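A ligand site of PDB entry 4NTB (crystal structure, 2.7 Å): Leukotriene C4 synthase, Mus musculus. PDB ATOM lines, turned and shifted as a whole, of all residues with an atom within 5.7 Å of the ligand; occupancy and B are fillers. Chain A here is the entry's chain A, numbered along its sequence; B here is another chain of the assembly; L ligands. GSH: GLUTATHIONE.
NE2 of Gln 59 of chain B is in hydrogen-bond range of OE2 of Glu 64 (2.8 Å). OD1 of Asn 61 sits close to OH of Tyr 99. The side-chain hydroxyl of Tyr 65 sits at hydrogen-bond distance from the side-chain hydroxyl of Ser 29 of chain B (3.0 Å). The backbone carbonyl oxygen (O) of Pro 44 of chain B lies within hydrogen-bond range of the guanidinium group (NH2) of Arg 36 of chain B, 3.3 Å away.
Merely in contact with the ligand: Ile 33 of chain B, Ser 29 of chain B, Phe 56 of chain B, Leu 114 and Val 32 of chain B. Hydrophobic or aromatic side chains within 4 Å of the ligand: Tyr 65, Tyr 99, Tyr 103, Leu 114, Val 32 of chain B, Ile 33 of chain B and Phe 56 of chain B. Of the 22 residues printed, 14 come within 4 Å of the ligand.
The side-chain amide nitrogen of Asn 61 sits at hydrogen-bond distance from an oxygen (O31) of the ligand (2.5 Å). O11 of the ligand lies within salt-bridge range of NH1 of Arg 36 of chain B (2.5 Å). O32 of the ligand is in salt-bridge range of NE of Arg 57, 3.0 Å away. The side-chain carboxylate (OE1) of Glu 64 is in salt-bridge range of a nitrogen (N1) of the ligand (2.9 Å). OH of Tyr 103 is in hydrogen-bond range of O32 of the ligand, at 3.1 Å. OE1 of Gln 59 of chain B is in hydrogen-bond range of N1 of the ligand. The side-chain hydroxyl of Tyr 99 sits at hydrogen-bond distance from an oxygen (O2) of the ligand, at 2.9 Å. The side-chain hydroxyl (OH) of Tyr 65 lies within hydrogen-bond range of an oxygen (OE1) of the ligand, at 2.7 Å. An oxygen (O2) of the ligand is in hydrogen-bond range of the guanidinium group (NH1) of Arg 110 (2.7 Å).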
ATOM      1  N   ARG A  57     -12.575  25.354  -4.737  1.00  0.00           N
ATOM      2  CA  ARG A  57     -13.267  24.557  -3.713  1.00  0.00           C
ATOM      3  C   ARG A  57     -13.559  25.363  -2.467  1.00  0.00           C
ATOM      4  O   ARG A  57     -14.586  25.140  -1.806  1.00  0.00           O
ATOM      5  CB  ARG A  57     -12.481  23.306  -3.351  1.00  0.00           C
ATOM      6  CG  ARG A  57     -12.255  22.342  -4.496  1.00  0.00           C
ATOM      7  CD  ARG A  57     -13.548  21.693  -4.980  1.00  0.00           C
ATOM      8  NE  ARG A  57     -14.483  21.452  -3.890  1.00  0.00           N
ATOM      9  CZ  ARG A  57     -15.767  21.144  -4.067  1.00  0.00           C
ATOM     10  NH1 ARG A  57     -16.254  21.020  -5.299  1.00  0.00           N
ATOM     11  NH2 ARG A  57     -16.555  20.962  -3.016  1.00  0.00           N
ATOM     12  N   ALA A  58     -12.671  26.292  -2.150  1.00  0.00           N
ATOM     13  CA  ALA A  58     -12.920  27.173  -1.021  1.00  0.00           C
ATOM     14  C   ALA A  58     -14.227  27.911  -1.258  1.00  0.00           C
ATOM     15  O   ALA A  58     -15.129  27.883  -0.412  1.00  0.00           O
ATOM     16  CB  ALA A  58     -11.767  28.153  -0.842  1.00  0.00           C
ATOM     17  N   VAL A  60     -16.701  27.253  -3.348  1.00  0.00           N
ATOM     18  CA  VAL A  60     -17.833  26.333  -3.389  1.00  0.00           C
ATOM     19  C   VAL A  60     -18.259  25.912  -1.992  1.00  0.00           C
ATOM     20  O   VAL A  60     -19.478  25.820  -1.706  1.00  0.00           O
ATOM     21  CB  VAL A  60     -17.499  25.048  -4.190  1.00  0.00           C
ATOM     22  CG1 VAL A  60     -18.484  23.932  -3.830  1.00  0.00           C
ATOM     23  CG2 VAL A  60     -17.513  25.323  -5.681  1.00  0.00           C
ATOM     24  N   ASN A  61     -17.263  25.666  -1.141  1.00  0.00           N
ATOM     25  CA  ASN A  61     -17.549  25.203   0.196  1.00  0.00           C
ATOM     26  C   ASN A  61     -18.322  26.279   0.929  1.00  0.00           C
ATOM     27  O   ASN A  61     -19.423  26.040   1.428  1.00  0.00           O
ATOM     28  CB  ASN A  61     -16.266  24.827   0.952  1.00  0.00           C
ATOM     29  CG  ASN A  61     -16.533  23.873   2.112  1.00  0.00           C
ATOM     30  OD1 ASN A  61     -16.745  24.286   3.262  1.00  0.00           O
ATOM     31  ND2 ASN A  61     -16.529  22.577   1.801  1.00  0.00           N
ATOM     32  N   GLU A  64     -21.923  26.941   0.024  1.00  0.00           N
ATOM     33  CA  GLU A  64     -22.770  25.814   0.367  1.00  0.00           C
ATOM     34  C   GLU A  64     -23.211  25.953   1.838  1.00  0.00           C
ATOM     35  O   GLU A  64     -24.320  25.587   2.200  1.00  0.00           O
ATOM     36  CB  GLU A  64     -21.888  24.607   0.269  1.00  0.00           C
ATOM     37  CG  GLU A  64     -22.546  23.316   0.060  1.00  0.00           C
ATOM     38  CD  GLU A  64     -21.480  22.263  -0.142  1.00  0.00           C
ATOM     39  OE1 GLU A  64     -20.549  22.237   0.701  1.00  0.00           O
ATOM     40  OE2 GLU A  64     -21.551  21.541  -1.150  1.00  0.00           O
ATOM     41  N   TYR A  65     -22.337  26.505   2.684  1.00  0.00           N
ATOM     42  CA  TYR A  65     -22.719  26.718   4.071  1.00  0.00           C
ATOM     43  C   TYR A  65     -23.424  28.030   4.249  1.00  0.00           C
ATOM     44  O   TYR A  65     -24.063  28.293   5.280  1.00  0.00           O
ATOM     45  CB  TYR A  65     -21.520  26.630   5.000  1.00  0.00           C
ATOM     46  CG  TYR A  65     -21.114  25.193   5.265  1.00  0.00           C
ATOM     47  CD1 TYR A  65     -20.268  24.513   4.393  1.00  0.00           C
ATOM     48  CD2 TYR A  65     -21.584  24.522   6.381  1.00  0.00           C
ATOM     49  CE1 TYR A  65     -19.896  23.218   4.629  1.00  0.00           C
ATOM     50  CE2 TYR A  65     -21.218  23.205   6.632  1.00  0.00           C
ATOM     51  CZ  TYR A  65     -20.368  22.560   5.750  1.00  0.00           C
ATOM     52  OH  TYR A  65     -19.996  21.265   5.986  1.00  0.00           O
ATOM     53  N   TYR A  99     -10.630  30.815   6.364  1.00  0.00           N
ATOM     54  CA  TYR A  99     -10.783  29.515   5.690  1.00  0.00           C
ATOM     55  C   TYR A  99     -10.393  29.633   4.222  1.00  0.00           C
ATOM     56  O   TYR A  99      -9.601  28.830   3.714  1.00  0.00           O
ATOM     57  CB  TYR A  99     -12.224  29.013   5.804  1.00  0.00           C
ATOM     58  CG  TYR A  99     -12.536  27.775   4.980  1.00  0.00           C
ATOM     59  CD1 TYR A  99     -12.250  26.495   5.457  1.00  0.00           C
ATOM     60  CD2 TYR A  99     -13.146  27.879   3.728  1.00  0.00           C
ATOM     61  CE1 TYR A  99     -12.544  25.359   4.699  1.00  0.00           C
ATOM     62  CE2 TYR A  99     -13.436  26.736   2.948  1.00  0.00           C
ATOM     63  CZ  TYR A  99     -13.135  25.475   3.446  1.00  0.00           C
ATOM     64  OH  TYR A  99     -13.423  24.355   2.689  1.00  0.00           O
ATOM     65  N   TYR A 103      -7.113  27.903   2.622  1.00  0.00           N
ATOM     66  CA  TYR A 103      -7.326  26.890   1.577  1.00  0.00           C
ATOM     67  C   TYR A 103      -6.532  27.206   0.312  1.00  0.00           C
ATOM     68  O   TYR A 103      -5.969  26.304  -0.302  1.00  0.00           O
ATOM     69  CB  TYR A 103      -8.813  26.820   1.228  1.00  0.00           C
ATOM     70  CG  TYR A 103      -9.268  25.493   0.686  1.00  0.00           C
ATOM     71  CD1 TYR A 103      -8.356  24.586   0.173  1.00  0.00           C
ATOM     72  CD2 TYR A 103     -10.611  25.138   0.685  1.00  0.00           C
ATOM     73  CE1 TYR A 103      -8.762  23.369  -0.327  1.00  0.00           C
ATOM     74  CE2 TYR A 103     -11.026  23.918   0.189  1.00  0.00           C
ATOM     75  CZ  TYR A 103     -10.090  23.033  -0.307  1.00  0.00           C
ATOM     76  OH  TYR A 103     -10.488  21.820  -0.812  1.00  0.00           O
ATOM     77  N   ARG A 110      -6.349  25.422   5.598  1.00  0.00           N
ATOM     78  CA  ARG A 110      -7.789  25.658   5.627  1.00  0.00           C
ATOM     79  C   ARG A 110      -8.433  25.147   6.921  1.00  0.00           C
ATOM     80  O   ARG A 110      -9.482  25.640   7.337  1.00  0.00           O
ATOM     81  CB  ARG A 110      -8.446  24.968   4.421  1.00  0.00           C
ATOM     82  CG  ARG A 110      -9.525  23.941   4.802  1.00  0.00           C
ATOM     83  CD  ARG A 110      -9.758  22.880   3.730  1.00  0.00           C
ATOM     84  NE  ARG A 110      -9.058  21.643   4.072  1.00  0.00           N
ATOM     85  CZ  ARG A 110      -9.640  20.473   4.320  1.00  0.00           C
ATOM     86  NH1 ARG A 110     -10.955  20.356   4.253  1.00  0.00           N
ATOM     87  NH2 ARG A 110      -8.910  19.409   4.645  1.00  0.00           N
ATOM     88  N   LEU A 111      -7.790  24.170   7.564  1.00  0.00           N
ATOM     89  CA  LEU A 111      -8.412  23.430   8.678  1.00  0.00           C
ATOM     90  C   LEU A 111      -8.652  24.253   9.948  1.00  0.00           C
ATOM     91  O   LEU A 111      -9.706  24.127  10.582  1.00  0.00           O
ATOM     92  CB  LEU A 111      -7.642  22.144   8.982  1.00  0.00           C
ATOM     93  CG  LEU A 111      -7.704  21.078   7.891  1.00  0.00           C
ATOM     94  CD1 LEU A 111      -6.634  20.003   8.059  1.00  0.00           C
ATOM     95  CD2 LEU A 111      -9.084  20.455   7.870  1.00  0.00           C
ATOM     96  N   LEU A 114     -11.613  26.600   9.403  1.00  0.00           N
ATOM     97  CA  LEU A 114     -12.809  25.775   9.237  1.00  0.00           C
ATOM     98  C   LEU A 114     -13.371  25.379  10.596  1.00  0.00           C
ATOM     99  O   LEU A 114     -14.587  25.448  10.845  1.00  0.00           O
ATOM    100  CB  LEU A 114     -12.482  24.511   8.437  1.00  0.00           C
ATOM    101  CG  LEU A 114     -13.629  23.502   8.298  1.00  0.00           C
ATOM    102  CD1 LEU A 114     -14.807  24.145   7.580  1.00  0.00           C
ATOM    103  CD2 LEU A 114     -13.160  22.271   7.548  1.00  0.00           C
ATOM    104  N   SER B  29     -23.400  16.796   5.420  1.00  0.00           N
ATOM    105  CA  SER B  29     -22.028  17.310   5.342  1.00  0.00           C
ATOM    106  C   SER B  29     -21.025  16.474   6.150  1.00  0.00           C
ATOM    107  O   SER B  29     -19.891  16.245   5.708  1.00  0.00           O
ATOM    108  CB  SER B  29     -21.984  18.761   5.798  1.00  0.00           C
ATOM    109  OG  SER B  29     -22.204  19.641   4.718  1.00  0.00           O
ATOM    110  N   LEU B  30     -21.450  16.023   7.338  1.00  0.00           N
ATOM    111  CA  LEU B  30     -20.630  15.136   8.167  1.00  0.00           C
ATOM    112  C   LEU B  30     -20.471  13.785   7.487  1.00  0.00           C
ATOM    113  O   LEU B  30     -19.379  13.192   7.527  1.00  0.00           O
ATOM    114  CB  LEU B  30     -21.216  15.003   9.589  1.00  0.00           C
ATOM    115  CG  LEU B  30     -21.163  16.263  10.481  1.00  0.00           C
ATOM    116  CD1 LEU B  30     -21.900  16.061  11.782  1.00  0.00           C
ATOM    117  CD2 LEU B  30     -19.737  16.788  10.753  1.00  0.00           C
ATOM    118  N   VAL B  32     -20.431  13.158   4.178  1.00  0.00           N
ATOM    119  CA  VAL B  32     -19.351  13.367   3.212  1.00  0.00           C
ATOM    120  C   VAL B  32     -17.965  13.339   3.875  1.00  0.00           C
ATOM    121  O   VAL B  32     -17.033  12.839   3.267  1.00  0.00           O
ATOM    122  CB  VAL B  32     -19.543  14.686   2.410  1.00  0.00           C
ATOM    123  CG1 VAL B  32     -18.397  14.916   1.402  1.00  0.00           C
ATOM    124  CG2 VAL B  32     -20.893  14.673   1.715  1.00  0.00           C
ATOM    125  N   ILE B  33     -17.802  13.861   5.098  1.00  0.00           N
ATOM    126  CA  ILE B  33     -16.489  13.858   5.777  1.00  0.00           C
ATOM    127  C   ILE B  33     -16.014  12.437   6.097  1.00  0.00           C
ATOM    128  O   ILE B  33     -14.825  12.130   5.915  1.00  0.00           O
ATOM    129  CB  ILE B  33     -16.445  14.645   7.112  1.00  0.00           C
ATOM    130  CG1 ILE B  33     -16.924  16.074   6.932  1.00  0.00           C
ATOM    131  CG2 ILE B  33     -15.008  14.694   7.655  1.00  0.00           C
ATOM    132  CD1 ILE B  33     -16.124  16.763   5.968  1.00  0.00           C
ATOM    133  N   ARG B  36     -15.172  10.617   2.943  1.00  0.00           N
ATOM    134  CA  ARG B  36     -13.942  11.257   2.468  1.00  0.00           C
ATOM    135  C   ARG B  36     -12.742  10.542   3.079  1.00  0.00           C
ATOM    136  O   ARG B  36     -11.682  10.409   2.444  1.00  0.00           O
ATOM    137  CB  ARG B  36     -13.976  12.725   2.899  1.00  0.00           C
ATOM    138  CG  ARG B  36     -13.160  13.649   2.077  1.00  0.00           C
ATOM    139  CD  ARG B  36     -13.955  14.852   1.590  1.00  0.00           C
ATOM    140  NE  ARG B  36     -13.265  15.410   0.423  1.00  0.00           N
ATOM    141  CZ  ARG B  36     -13.814  16.222  -0.469  1.00  0.00           C
ATOM    142  NH1 ARG B  36     -15.082  16.590  -0.350  1.00  0.00           N
ATOM    143  NH2 ARG B  36     -13.101  16.674  -1.482  1.00  0.00           N
ATOM    144  N   PRO B  43      -9.203  16.480   0.307  1.00  0.00           N
ATOM    145  CA  PRO B  43      -9.419  17.806  -0.301  1.00  0.00           C
ATOM    146  C   PRO B  43      -8.147  18.402  -0.965  1.00  0.00           C
ATOM    147  O   PRO B  43      -7.074  18.328  -0.370  1.00  0.00           O
ATOM    148  CB  PRO B  43      -9.924  18.661   0.865  1.00  0.00           C
ATOM    149  CG  PRO B  43     -10.585  17.672   1.780  1.00  0.00           C
ATOM    150  CD  PRO B  43      -9.742  16.418   1.686  1.00  0.00           C
ATOM    151  N   PRO B  44      -8.269  18.969  -2.183  1.00  0.00           N
ATOM    152  CA  PRO B  44      -9.526  19.103  -2.956  1.00  0.00           C
ATOM    153  C   PRO B  44      -9.945  17.760  -3.557  1.00  0.00           C
ATOM    154  O   PRO B  44     -10.111  16.815  -2.801  1.00  0.00           O
ATOM    155  CB  PRO B  44      -9.179  20.142  -4.033  1.00  0.00           C
ATOM    156  CG  PRO B  44      -7.679  20.091  -4.177  1.00  0.00           C
ATOM    157  CD  PRO B  44      -7.129  19.618  -2.855  1.00  0.00           C
ATOM    158  N   THR B  46     -12.890  15.899  -5.910  1.00  0.00           N
ATOM    159  CA  THR B  46     -14.258  15.511  -5.609  1.00  0.00           C
ATOM    160  C   THR B  46     -14.606  14.196  -6.330  1.00  0.00           C
ATOM    161  O   THR B  46     -15.775  13.879  -6.544  1.00  0.00           O
ATOM    162  CB  THR B  46     -15.254  16.651  -5.932  1.00  0.00           C
ATOM    163  OG1 THR B  46     -15.101  17.058  -7.296  1.00  0.00           O
ATOM    164  CG2 THR B  46     -14.997  17.851  -5.035  1.00  0.00           C
ATOM    165  N   PHE B  56     -21.070  12.256  -2.184  1.00  0.00           N
ATOM    166  CA  PHE B  56     -20.762  13.643  -2.527  1.00  0.00           C
ATOM    167  C   PHE B  56     -21.947  14.290  -3.256  1.00  0.00           C
ATOM    168  O   PHE B  56     -22.347  15.419  -2.918  1.00  0.00           O
ATOM    169  CB  PHE B  56     -19.476  13.738  -3.383  1.00  0.00           C
ATOM    170  CG  PHE B  56     -19.150  15.130  -3.853  1.00  0.00           C
ATOM    171  CD1 PHE B  56     -18.742  16.122  -2.955  1.00  0.00           C
ATOM    172  CD2 PHE B  56     -19.258  15.458  -5.207  1.00  0.00           C
ATOM    173  CE1 PHE B  56     -18.435  17.415  -3.396  1.00  0.00           C
ATOM    174  CE2 PHE B  56     -18.950  16.757  -5.664  1.00  0.00           C
ATOM    175  CZ  PHE B  56     -18.540  17.730  -4.754  1.00  0.00           C
ATOM    176  N   GLN B  59     -25.268  14.994  -1.233  1.00  0.00           N
ATOM    177  CA  GLN B  59     -25.070  16.187  -0.411  1.00  0.00           C
ATOM    178  C   GLN B  59     -25.195  17.464  -1.229  1.00  0.00           C
ATOM    179  O   GLN B  59     -25.901  18.418  -0.812  1.00  0.00           O
ATOM    180  CB  GLN B  59     -23.689  16.148   0.236  1.00  0.00           C
ATOM    181  CG  GLN B  59     -23.370  17.332   1.126  1.00  0.00           C
ATOM    182  CD  GLN B  59     -22.469  18.350   0.429  1.00  0.00           C
ATOM    183  OE1 GLN B  59     -21.313  18.043   0.064  1.00  0.00           O
ATOM    184  NE2 GLN B  59     -22.987  19.584   0.256  1.00  0.00           N
ATOM    185  N   VAL B  60     -24.521  17.469  -2.383  1.00  0.00           N
ATOM    186  CA  VAL B  60     -24.529  18.622  -3.278  1.00  0.00           C
ATOM    187  C   VAL B  60     -25.924  18.900  -3.813  1.00  0.00           C
ATOM    188  O   VAL B  60     -26.337  20.082  -3.910  1.00  0.00           O
ATOM    189  CB  VAL B  60     -23.588  18.411  -4.493  1.00  0.00           C
ATOM    190  CG1 VAL B  60     -23.961  19.377  -5.621  1.00  0.00           C
ATOM    191  CG2 VAL B  60     -22.138  18.584  -4.088  1.00  0.00           C
HETATM  192  N1  GSH L   1     -18.977  19.877   0.238  1.00  0.00           N
HETATM  193  CA1 GSH L   1     -18.136  19.432   1.334  1.00  0.00           C
HETATM  194  C1  GSH L   1     -17.022  18.503   0.804  1.00  0.00           C
HETATM  195  O11 GSH L   1     -16.993  18.139  -0.410  1.00  0.00           O
HETATM  196  O12 GSH L   1     -16.093  18.081   1.575  1.00  0.00           O
HETATM  197  CB1 GSH L   1     -19.039  18.784   2.361  1.00  0.00           C
HETATM  198  CG1 GSH L   1     -18.354  18.452   3.706  1.00  0.00           C
HETATM  199  CD1 GSH L   1     -17.324  19.469   4.255  1.00  0.00           C
HETATM  200  OE1 GSH L   1     -17.705  20.474   4.794  1.00  0.00           O
HETATM  201  N2  GSH L   1     -15.899  19.204   4.152  1.00  0.00           N
HETATM  202  CA2 GSH L   1     -14.900  20.115   4.701  1.00  0.00           C
HETATM  203  C2  GSH L   1     -14.036  20.767   3.622  1.00  0.00           C
HETATM  204  O2  GSH L   1     -13.326  21.704   3.946  1.00  0.00           O
HETATM  205  CB2 GSH L   1     -13.973  19.423   5.659  1.00  0.00           C
HETATM  206  SG2 GSH L   1     -13.159  17.985   5.012  1.00  0.00           S
HETATM  207  N3  GSH L   1     -14.083  20.269   2.294  1.00  0.00           N
HETATM  208  CA3 GSH L   1     -13.278  20.855   1.259  1.00  0.00           C
HETATM  209  C3  GSH L   1     -14.062  21.090  -0.026  1.00  0.00           C
HETATM  210  O31 GSH L   1     -15.279  21.469  -0.011  1.00  0.00           O
HETATM  211  O32 GSH L   1     -13.452  20.926  -1.132  1.00  0.00           O
